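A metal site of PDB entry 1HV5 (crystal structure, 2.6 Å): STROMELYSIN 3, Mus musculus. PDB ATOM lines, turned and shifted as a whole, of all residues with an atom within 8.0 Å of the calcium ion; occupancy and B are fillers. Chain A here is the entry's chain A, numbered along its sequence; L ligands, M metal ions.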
ATOM      1  N   ALA A  64      22.584  -0.659  10.957  1.00  0.00           N
ATOM      2  CA  ALA A  64      21.369  -1.490  10.896  1.00  0.00           C
ATOM      3  C   ALA A  64      20.858  -1.617   9.466  1.00  0.00           C
ATOM      4  O   ALA A  64      21.282  -0.897   8.560  1.00  0.00           O
ATOM      5  CB  ALA A  64      20.269  -0.852  11.746  1.00  0.00           C
ATOM      6  N   TYR A  66      17.287  -2.202   7.084  1.00  0.00           N
ATOM      7  CA  TYR A  66      15.855  -2.067   6.846  1.00  0.00           C
ATOM      8  C   TYR A  66      15.163  -1.346   8.008  1.00  0.00           C
ATOM      9  O   TYR A  66      15.724  -0.382   8.569  1.00  0.00           O
ATOM     10  CB  TYR A  66      15.276  -3.463   6.650  1.00  0.00           C
ATOM     11  CG  TYR A  66      15.558  -4.000   5.254  1.00  0.00           C
ATOM     12  CD1 TYR A  66      16.590  -4.935   5.038  1.00  0.00           C
ATOM     13  CD2 TYR A  66      14.787  -3.553   4.179  1.00  0.00           C
ATOM     14  CE1 TYR A  66      16.849  -5.400   3.745  1.00  0.00           C
ATOM     15  CE2 TYR A  66      15.052  -3.999   2.886  1.00  0.00           C
ATOM     16  CZ  TYR A  66      16.089  -4.925   2.660  1.00  0.00           C
ATOM     17  OH  TYR A  66      16.357  -5.351   1.397  1.00  0.00           O
ATOM     18  N   PRO A  73      13.170   3.109   7.936  1.00  0.00           N
ATOM     19  CA  PRO A  73      13.737   1.857   7.483  1.00  0.00           C
ATOM     20  C   PRO A  73      14.746   2.095   6.409  1.00  0.00           C
ATOM     21  O   PRO A  73      14.517   3.002   5.555  1.00  0.00           O
ATOM     22  CB  PRO A  73      12.580   1.134   6.827  1.00  0.00           C
ATOM     23  CG  PRO A  73      11.382   2.066   6.876  1.00  0.00           C
ATOM     24  CD  PRO A  73      11.750   3.304   7.636  1.00  0.00           C
ATOM     25  N   PHE A  74      15.813   1.328   6.412  1.00  0.00           N
ATOM     26  CA  PHE A  74      16.815   1.430   5.335  1.00  0.00           C
ATOM     27  C   PHE A  74      16.280   0.618   4.142  1.00  0.00           C
ATOM     28  O   PHE A  74      15.285  -0.113   4.272  1.00  0.00           O
ATOM     29  CB  PHE A  74      18.180   0.926   5.796  1.00  0.00           C
ATOM     30  CG  PHE A  74      18.946   1.963   6.637  1.00  0.00           C
ATOM     31  CD1 PHE A  74      19.101   3.281   6.185  1.00  0.00           C
ATOM     32  CD2 PHE A  74      19.510   1.581   7.860  1.00  0.00           C
ATOM     33  CE1 PHE A  74      19.816   4.210   6.964  1.00  0.00           C
ATOM     34  CE2 PHE A  74      20.212   2.503   8.637  1.00  0.00           C
ATOM     35  CZ  PHE A  74      20.366   3.822   8.194  1.00  0.00           C
ATOM     36  N   ASP A  75      16.935   0.742   3.000  1.00  0.00           N
ATOM     37  CA  ASP A  75      16.449   0.125   1.753  1.00  0.00           C
ATOM     38  C   ASP A  75      17.427  -0.831   1.053  1.00  0.00           C
ATOM     39  O   ASP A  75      17.375  -1.022  -0.170  1.00  0.00           O
ATOM     40  CB  ASP A  75      16.168   1.223   0.728  1.00  0.00           C
ATOM     41  CG  ASP A  75      17.347   2.195   0.613  1.00  0.00           C
ATOM     42  OD1 ASP A  75      18.513   1.838   1.035  1.00  0.00           O
ATOM     43  OD2 ASP A  75      17.173   3.358   0.108  1.00  0.00           O
ATOM     44  N   GLY A  76      18.316  -1.459   1.812  1.00  0.00           N
ATOM     45  CA  GLY A  76      19.282  -2.422   1.232  1.00  0.00           C
ATOM     46  C   GLY A  76      20.391  -1.688   0.451  1.00  0.00           C
ATOM     47  O   GLY A  76      20.542  -0.465   0.560  1.00  0.00           O
ATOM     48  N   PRO A  77      21.212  -2.394  -0.367  1.00  0.00           N
ATOM     49  CA  PRO A  77      22.312  -1.775  -1.092  1.00  0.00           C
ATOM     50  C   PRO A  77      21.857  -0.582  -1.906  1.00  0.00           C
ATOM     51  O   PRO A  77      20.769  -0.647  -2.556  1.00  0.00           O
ATOM     52  CB  PRO A  77      22.909  -2.909  -1.902  1.00  0.00           C
ATOM     53  CG  PRO A  77      22.153  -4.177  -1.554  1.00  0.00           C
ATOM     54  CD  PRO A  77      21.054  -3.838  -0.597  1.00  0.00           C
ATOM     55  N   GLY A  78      22.669   0.473  -1.848  1.00  0.00           N
ATOM     56  CA  GLY A  78      22.393   1.727  -2.567  1.00  0.00           C
ATOM     57  C   GLY A  78      21.290   2.527  -1.858  1.00  0.00           C
ATOM     58  O   GLY A  78      20.954   2.253  -0.689  1.00  0.00           O
ATOM     59  N   GLY A  79      20.737   3.500  -2.573  1.00  0.00           N
ATOM     60  CA  GLY A  79      19.679   4.369  -2.033  1.00  0.00           C
ATOM     61  C   GLY A  79      20.256   5.165  -0.863  1.00  0.00           C
ATOM     62  O   GLY A  79      21.294   5.838  -0.993  1.00  0.00           O
ATOM     63  N   ILE A  80      19.585   5.079   0.265  1.00  0.00           N
ATOM     64  CA  ILE A  80      20.064   5.752   1.487  1.00  0.00           C
ATOM     65  C   ILE A  80      21.221   4.940   2.054  1.00  0.00           C
ATOM     66  O   ILE A  80      21.195   3.703   2.056  1.00  0.00           O
ATOM     67  CB  ILE A  80      18.944   5.843   2.526  1.00  0.00           C
ATOM     68  CG1 ILE A  80      17.694   6.540   2.002  1.00  0.00           C
ATOM     69  CG2 ILE A  80      19.368   6.643   3.774  1.00  0.00           C
ATOM     70  CD1 ILE A  80      17.973   7.941   1.452  1.00  0.00           C
ATOM     71  N   LEU A  81      22.226   5.656   2.514  1.00  0.00           N
ATOM     72  CA  LEU A  81      23.433   5.028   3.058  1.00  0.00           C
ATOM     73  C   LEU A  81      23.467   5.161   4.576  1.00  0.00           C
ATOM     74  O   LEU A  81      24.110   4.367   5.275  1.00  0.00           O
ATOM     75  CB  LEU A  81      24.657   5.697   2.471  1.00  0.00           C
ATOM     76  CG  LEU A  81      24.552   5.868   0.956  1.00  0.00           C
ATOM     77  CD1 LEU A  81      25.679   6.722   0.384  1.00  0.00           C
ATOM     78  CD2 LEU A  81      24.588   4.534   0.213  1.00  0.00           C
ATOM     79  N   ALA A  82      22.778   6.159   5.065  1.00  0.00           N
ATOM     80  CA  ALA A  82      22.707   6.438   6.498  1.00  0.00           C
ATOM     81  C   ALA A  82      21.813   7.641   6.741  1.00  0.00           C
ATOM     82  O   ALA A  82      21.350   8.283   5.804  1.00  0.00           O
ATOM     83  CB  ALA A  82      24.117   6.758   7.021  1.00  0.00           C
ATOM     84  N   PHE A  97      24.057   3.842  10.058  1.00  0.00           N
ATOM     85  CA  PHE A  97      24.597   3.539   8.729  1.00  0.00           C
ATOM     86  C   PHE A  97      23.895   2.286   8.243  1.00  0.00           C
ATOM     87  O   PHE A  97      23.662   1.357   9.037  1.00  0.00           O
ATOM     88  CB  PHE A  97      26.091   3.265   8.811  1.00  0.00           C
ATOM     89  CG  PHE A  97      26.880   4.487   9.231  1.00  0.00           C
ATOM     90  CD1 PHE A  97      27.397   5.343   8.261  1.00  0.00           C
ATOM     91  CD2 PHE A  97      27.083   4.739  10.586  1.00  0.00           C
ATOM     92  CE1 PHE A  97      28.115   6.473   8.645  1.00  0.00           C
ATOM     93  CE2 PHE A  97      27.790   5.873  10.978  1.00  0.00           C
ATOM     94  CZ  PHE A  97      28.305   6.751  10.007  1.00  0.00           C
ATOM     95  N   ASP A  98      23.558   2.264   6.966  1.00  0.00           N
ATOM     96  CA  ASP A  98      22.882   1.098   6.388  1.00  0.00           C
ATOM     97  C   ASP A  98      23.913  -0.029   6.264  1.00  0.00           C
ATOM     98  O   ASP A  98      24.855   0.052   5.492  1.00  0.00           O
ATOM     99  CB  ASP A  98      22.326   1.423   4.998  1.00  0.00           C
ATOM    100  CG  ASP A  98      21.423   0.330   4.452  1.00  0.00           C
ATOM    101  OD1 ASP A  98      21.511  -0.834   4.894  1.00  0.00           O
ATOM    102  OD2 ASP A  98      20.620   0.628   3.553  1.00  0.00           O
ATOM    103  N   TYR A  99      23.718  -1.056   7.069  1.00  0.00           N
ATOM    104  CA  TYR A  99      24.554  -2.228   7.099  1.00  0.00           C
ATOM    105  C   TYR A  99      24.663  -2.904   5.724  1.00  0.00           C
ATOM    106  O   TYR A  99      25.657  -3.569   5.427  1.00  0.00           O
ATOM    107  CB  TYR A  99      23.976  -3.190   8.137  1.00  0.00           C
ATOM    108  CG  TYR A  99      24.727  -4.480   8.342  1.00  0.00           C
ATOM    109  CD1 TYR A  99      24.293  -5.651   7.731  1.00  0.00           C
ATOM    110  CD2 TYR A  99      25.833  -4.539   9.185  1.00  0.00           C
ATOM    111  CE1 TYR A  99      24.939  -6.860   7.967  1.00  0.00           C
ATOM    112  CE2 TYR A  99      26.487  -5.729   9.421  1.00  0.00           C
ATOM    113  CZ  TYR A  99      26.033  -6.893   8.816  1.00  0.00           C
ATOM    114  OH  TYR A  99      26.670  -8.088   9.070  1.00  0.00           O
ATOM    115  N   ASP A 100      23.675  -2.708   4.862  1.00  0.00           N
ATOM    116  CA  ASP A 100      23.725  -3.363   3.558  1.00  0.00           C
ATOM    117  C   ASP A 100      24.641  -2.792   2.483  1.00  0.00           C
ATOM    118  O   ASP A 100      24.751  -3.363   1.385  1.00  0.00           O
ATOM    119  CB  ASP A 100      22.330  -3.497   2.976  1.00  0.00           C
ATOM    120  CG  ASP A 100      21.468  -4.439   3.755  1.00  0.00           C
ATOM    121  OD1 ASP A 100      22.002  -5.383   4.395  1.00  0.00           O
ATOM    122  OD2 ASP A 100      20.235  -4.251   3.728  1.00  0.00           O
ATOM    123  N   GLU A 101      25.311  -1.687   2.779  1.00  0.00           N
ATOM    124  CA  GLU A 101      26.194  -1.114   1.779  1.00  0.00           C
ATOM    125  C   GLU A 101      27.537  -1.823   1.802  1.00  0.00           C
ATOM    126  O   GLU A 101      27.901  -2.482   2.785  1.00  0.00           O
ATOM    127  CB  GLU A 101      26.447   0.369   2.042  1.00  0.00           C
ATOM    128  CG  GLU A 101      25.236   1.178   2.339  1.00  0.00           C
ATOM    129  CD  GLU A 101      24.193   1.149   1.258  1.00  0.00           C
ATOM    130  OE1 GLU A 101      24.549   1.138   0.057  1.00  0.00           O
ATOM    131  OE2 GLU A 101      22.994   1.164   1.599  1.00  0.00           O
ATOM    132  N   TRP A 103      30.688  -1.207   2.507  1.00  0.00           N
ATOM    133  CA  TRP A 103      31.489  -0.193   3.162  1.00  0.00           C
ATOM    134  C   TRP A 103      32.986  -0.307   2.882  1.00  0.00           C
ATOM    135  O   TRP A 103      33.572  -1.388   2.991  1.00  0.00           O
ATOM    136  CB  TRP A 103      31.220  -0.215   4.662  1.00  0.00           C
ATOM    137  CG  TRP A 103      29.813   0.186   4.971  1.00  0.00           C
ATOM    138  CD1 TRP A 103      28.785  -0.619   5.384  1.00  0.00           C
ATOM    139  CD2 TRP A 103      29.280   1.502   4.869  1.00  0.00           C
ATOM    140  NE1 TRP A 103      27.647   0.120   5.543  1.00  0.00           N
ATOM    141  CE2 TRP A 103      27.923   1.426   5.241  1.00  0.00           C
ATOM    142  CE3 TRP A 103      29.805   2.748   4.497  1.00  0.00           C
ATOM    143  CZ2 TRP A 103      27.091   2.543   5.256  1.00  0.00           C
ATOM    144  CZ3 TRP A 103      28.984   3.840   4.514  1.00  0.00           C
ATOM    145  CH2 TRP A 103      27.639   3.738   4.890  1.00  0.00           C
HETATM  146  N1  LIG L   1      23.378   7.705  -2.121  1.00  0.00           N
HETATM  147  N2  LIG L   1      21.964  10.044   0.048  1.00  0.00           N
HETATM  148  C1  LIG L   1      21.740   9.341  -1.215  1.00  0.00           C
HETATM  149  C2  LIG L   1      20.645  10.066  -2.011  1.00  0.00           C
HETATM  150  C3  LIG L   1      20.227   9.211  -3.164  1.00  0.00           C
HETATM  151  C4  LIG L   1      19.166   8.334  -3.087  1.00  0.00           C
HETATM  152  C5  LIG L   1      20.829   9.141  -4.475  1.00  0.00           C
HETATM  153  N3  LIG L   1      20.169   8.193  -5.235  1.00  0.00           N
HETATM  154  C6  LIG L   1      19.129   7.658  -4.495  1.00  0.00           C
HETATM  155  C7  LIG L   1      18.166   7.954  -2.055  1.00  0.00           C
HETATM  156  C8  LIG L   1      18.151   6.634  -4.894  1.00  0.00           C
HETATM  157  C9  LIG L   1      17.116   6.946  -2.446  1.00  0.00           C
HETATM  158  C10 LIG L   1      17.099   6.284  -3.871  1.00  0.00           C
HETATM  159  C11 LIG L   1      23.159   9.021  -1.851  1.00  0.00           C
HETATM  160  O1  LIG L   1      23.821  10.004  -2.147  1.00  0.00           O
HETATM  161  O2  LIG L   1      21.976   8.362   1.377  1.00  0.00           O
HETATM  162  C12 LIG L   1      22.095   9.512   1.272  1.00  0.00           C
HETATM  163  C13 LIG L   1      23.420  10.095   3.461  1.00  0.00           C
HETATM  164  C14 LIG L   1      26.602  11.856   1.697  1.00  0.00           C
HETATM  165  C15 LIG L   1      26.688  13.074   0.935  1.00  0.00           C
HETATM  166  C16 LIG L   1      28.027  13.614   0.655  1.00  0.00           C
HETATM  167  C17 LIG L   1      29.251  12.949   1.083  1.00  0.00           C
HETATM  168  C18 LIG L   1      29.138  11.667   1.743  1.00  0.00           C
HETATM  169  C19 LIG L   1      27.842  11.025   2.054  1.00  0.00           C
HETATM  170  C20 LIG L   1      22.287  10.419   2.529  1.00  0.00           C
HETATM  171  C21 LIG L   1      24.749  10.469   2.885  1.00  0.00           C
HETATM  172  C22 LIG L   1      25.188  11.674   1.986  1.00  0.00           C
HETATM  173  C23 LIG L   1      21.055  10.274   3.462  1.00  0.00           C
HETATM  174  P1  LIG L   1      20.740  11.549   4.631  1.00  0.00           P
HETATM  175  O3  LIG L   1      20.870  12.590   3.855  1.00  0.00           O
HETATM  176  O4  LIG L   1      21.493  11.727   5.710  1.00  0.00           O
HETATM  177  N4  LIG L   1      18.187  11.341   4.087  1.00  0.00           N
HETATM  178  C24 LIG L   1      19.043  11.459   5.256  1.00  0.00           C
HETATM  179  C25 LIG L   1      18.559  12.744   5.983  1.00  0.00           C
HETATM  180  C26 LIG L   1      17.486  12.530   6.914  1.00  0.00           C
HETATM  181  C27 LIG L   1      15.992  12.464   6.485  1.00  0.00           C
HETATM  182  C28 LIG L   1      17.831  12.335   8.366  1.00  0.00           C
HETATM  183  C29 LIG L   1      14.900  12.193   7.406  1.00  0.00           C
HETATM  184  C30 LIG L   1      16.715  12.073   9.323  1.00  0.00           C
HETATM  185  C31 LIG L   1      15.277  12.008   8.821  1.00  0.00           C
HETATM  186  C32 LIG L   1      16.954  10.774   3.634  1.00  0.00           C
HETATM  187  O5  LIG L   1      16.437  11.245   2.455  1.00  0.00           O
HETATM  188  O6  LIG L   1      16.295   9.906   4.654  1.00  0.00           O
HETATM  189  C33 LIG L   1      14.829   9.413   4.394  1.00  0.00           C
HETATM  190  C34 LIG L   1      13.819  10.364   3.590  1.00  0.00           C
HETATM  191  C35 LIG L   1      13.235  11.664   4.179  1.00  0.00           C
HETATM  192  C36 LIG L   1      12.564  12.714   3.249  1.00  0.00           C
HETATM  193  C37 LIG L   1      12.387  12.421   1.718  1.00  0.00           C
HETATM  194  C38 LIG L   1      12.847  11.080   1.071  1.00  0.00           C
HETATM  195  C39 LIG L   1      13.607  10.094   2.062  1.00  0.00           C
HETATM  196 CA    CA M   1      20.691   1.535   1.285  1.00  0.00          CA
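The calcium ion is bound by the backbone carbonyl oxygen of Gly 78 (2.1 Å), the backbone carbonyl oxygen of Gly 76 (2.1 Å), the side-chain carboxylate of Asp 75 (2.2 Å), the side-chain carboxylate of Glu 101 (2.4 Å), the backbone carbonyl oxygen of Ile 80 (2.4 Å) and the side-chain carboxylate of Asp 98 (2.4 Å).
Six residues have an atom within 4 Å of the calcium ion: Asp 75, Gly 76, Gly 78, Ile 80, Asp 98 and Glu 101.
The backbone carbonyl oxygen (O) of Gly 79 lies within hydrogen-bond range of a nitrogen (N1) of the ligand, 3.0 Å away. The backbone NH (N) of Leu 81 sits at hydrogen-bond distance from an oxygen (O2) of the ligand (2.9 Å).
The backbone NH of Asp 98 is in hydrogen-bond range of the backbone carbonyl oxygen of Leu 81 (2.8 Å). N of Asp 100 lies within hydrogen-bond range of OD1 of Asp 98 (2.9 Å). O of Asp 98 lies within hydrogen-bond range of NE1 of Trp 103 (2.8 Å).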
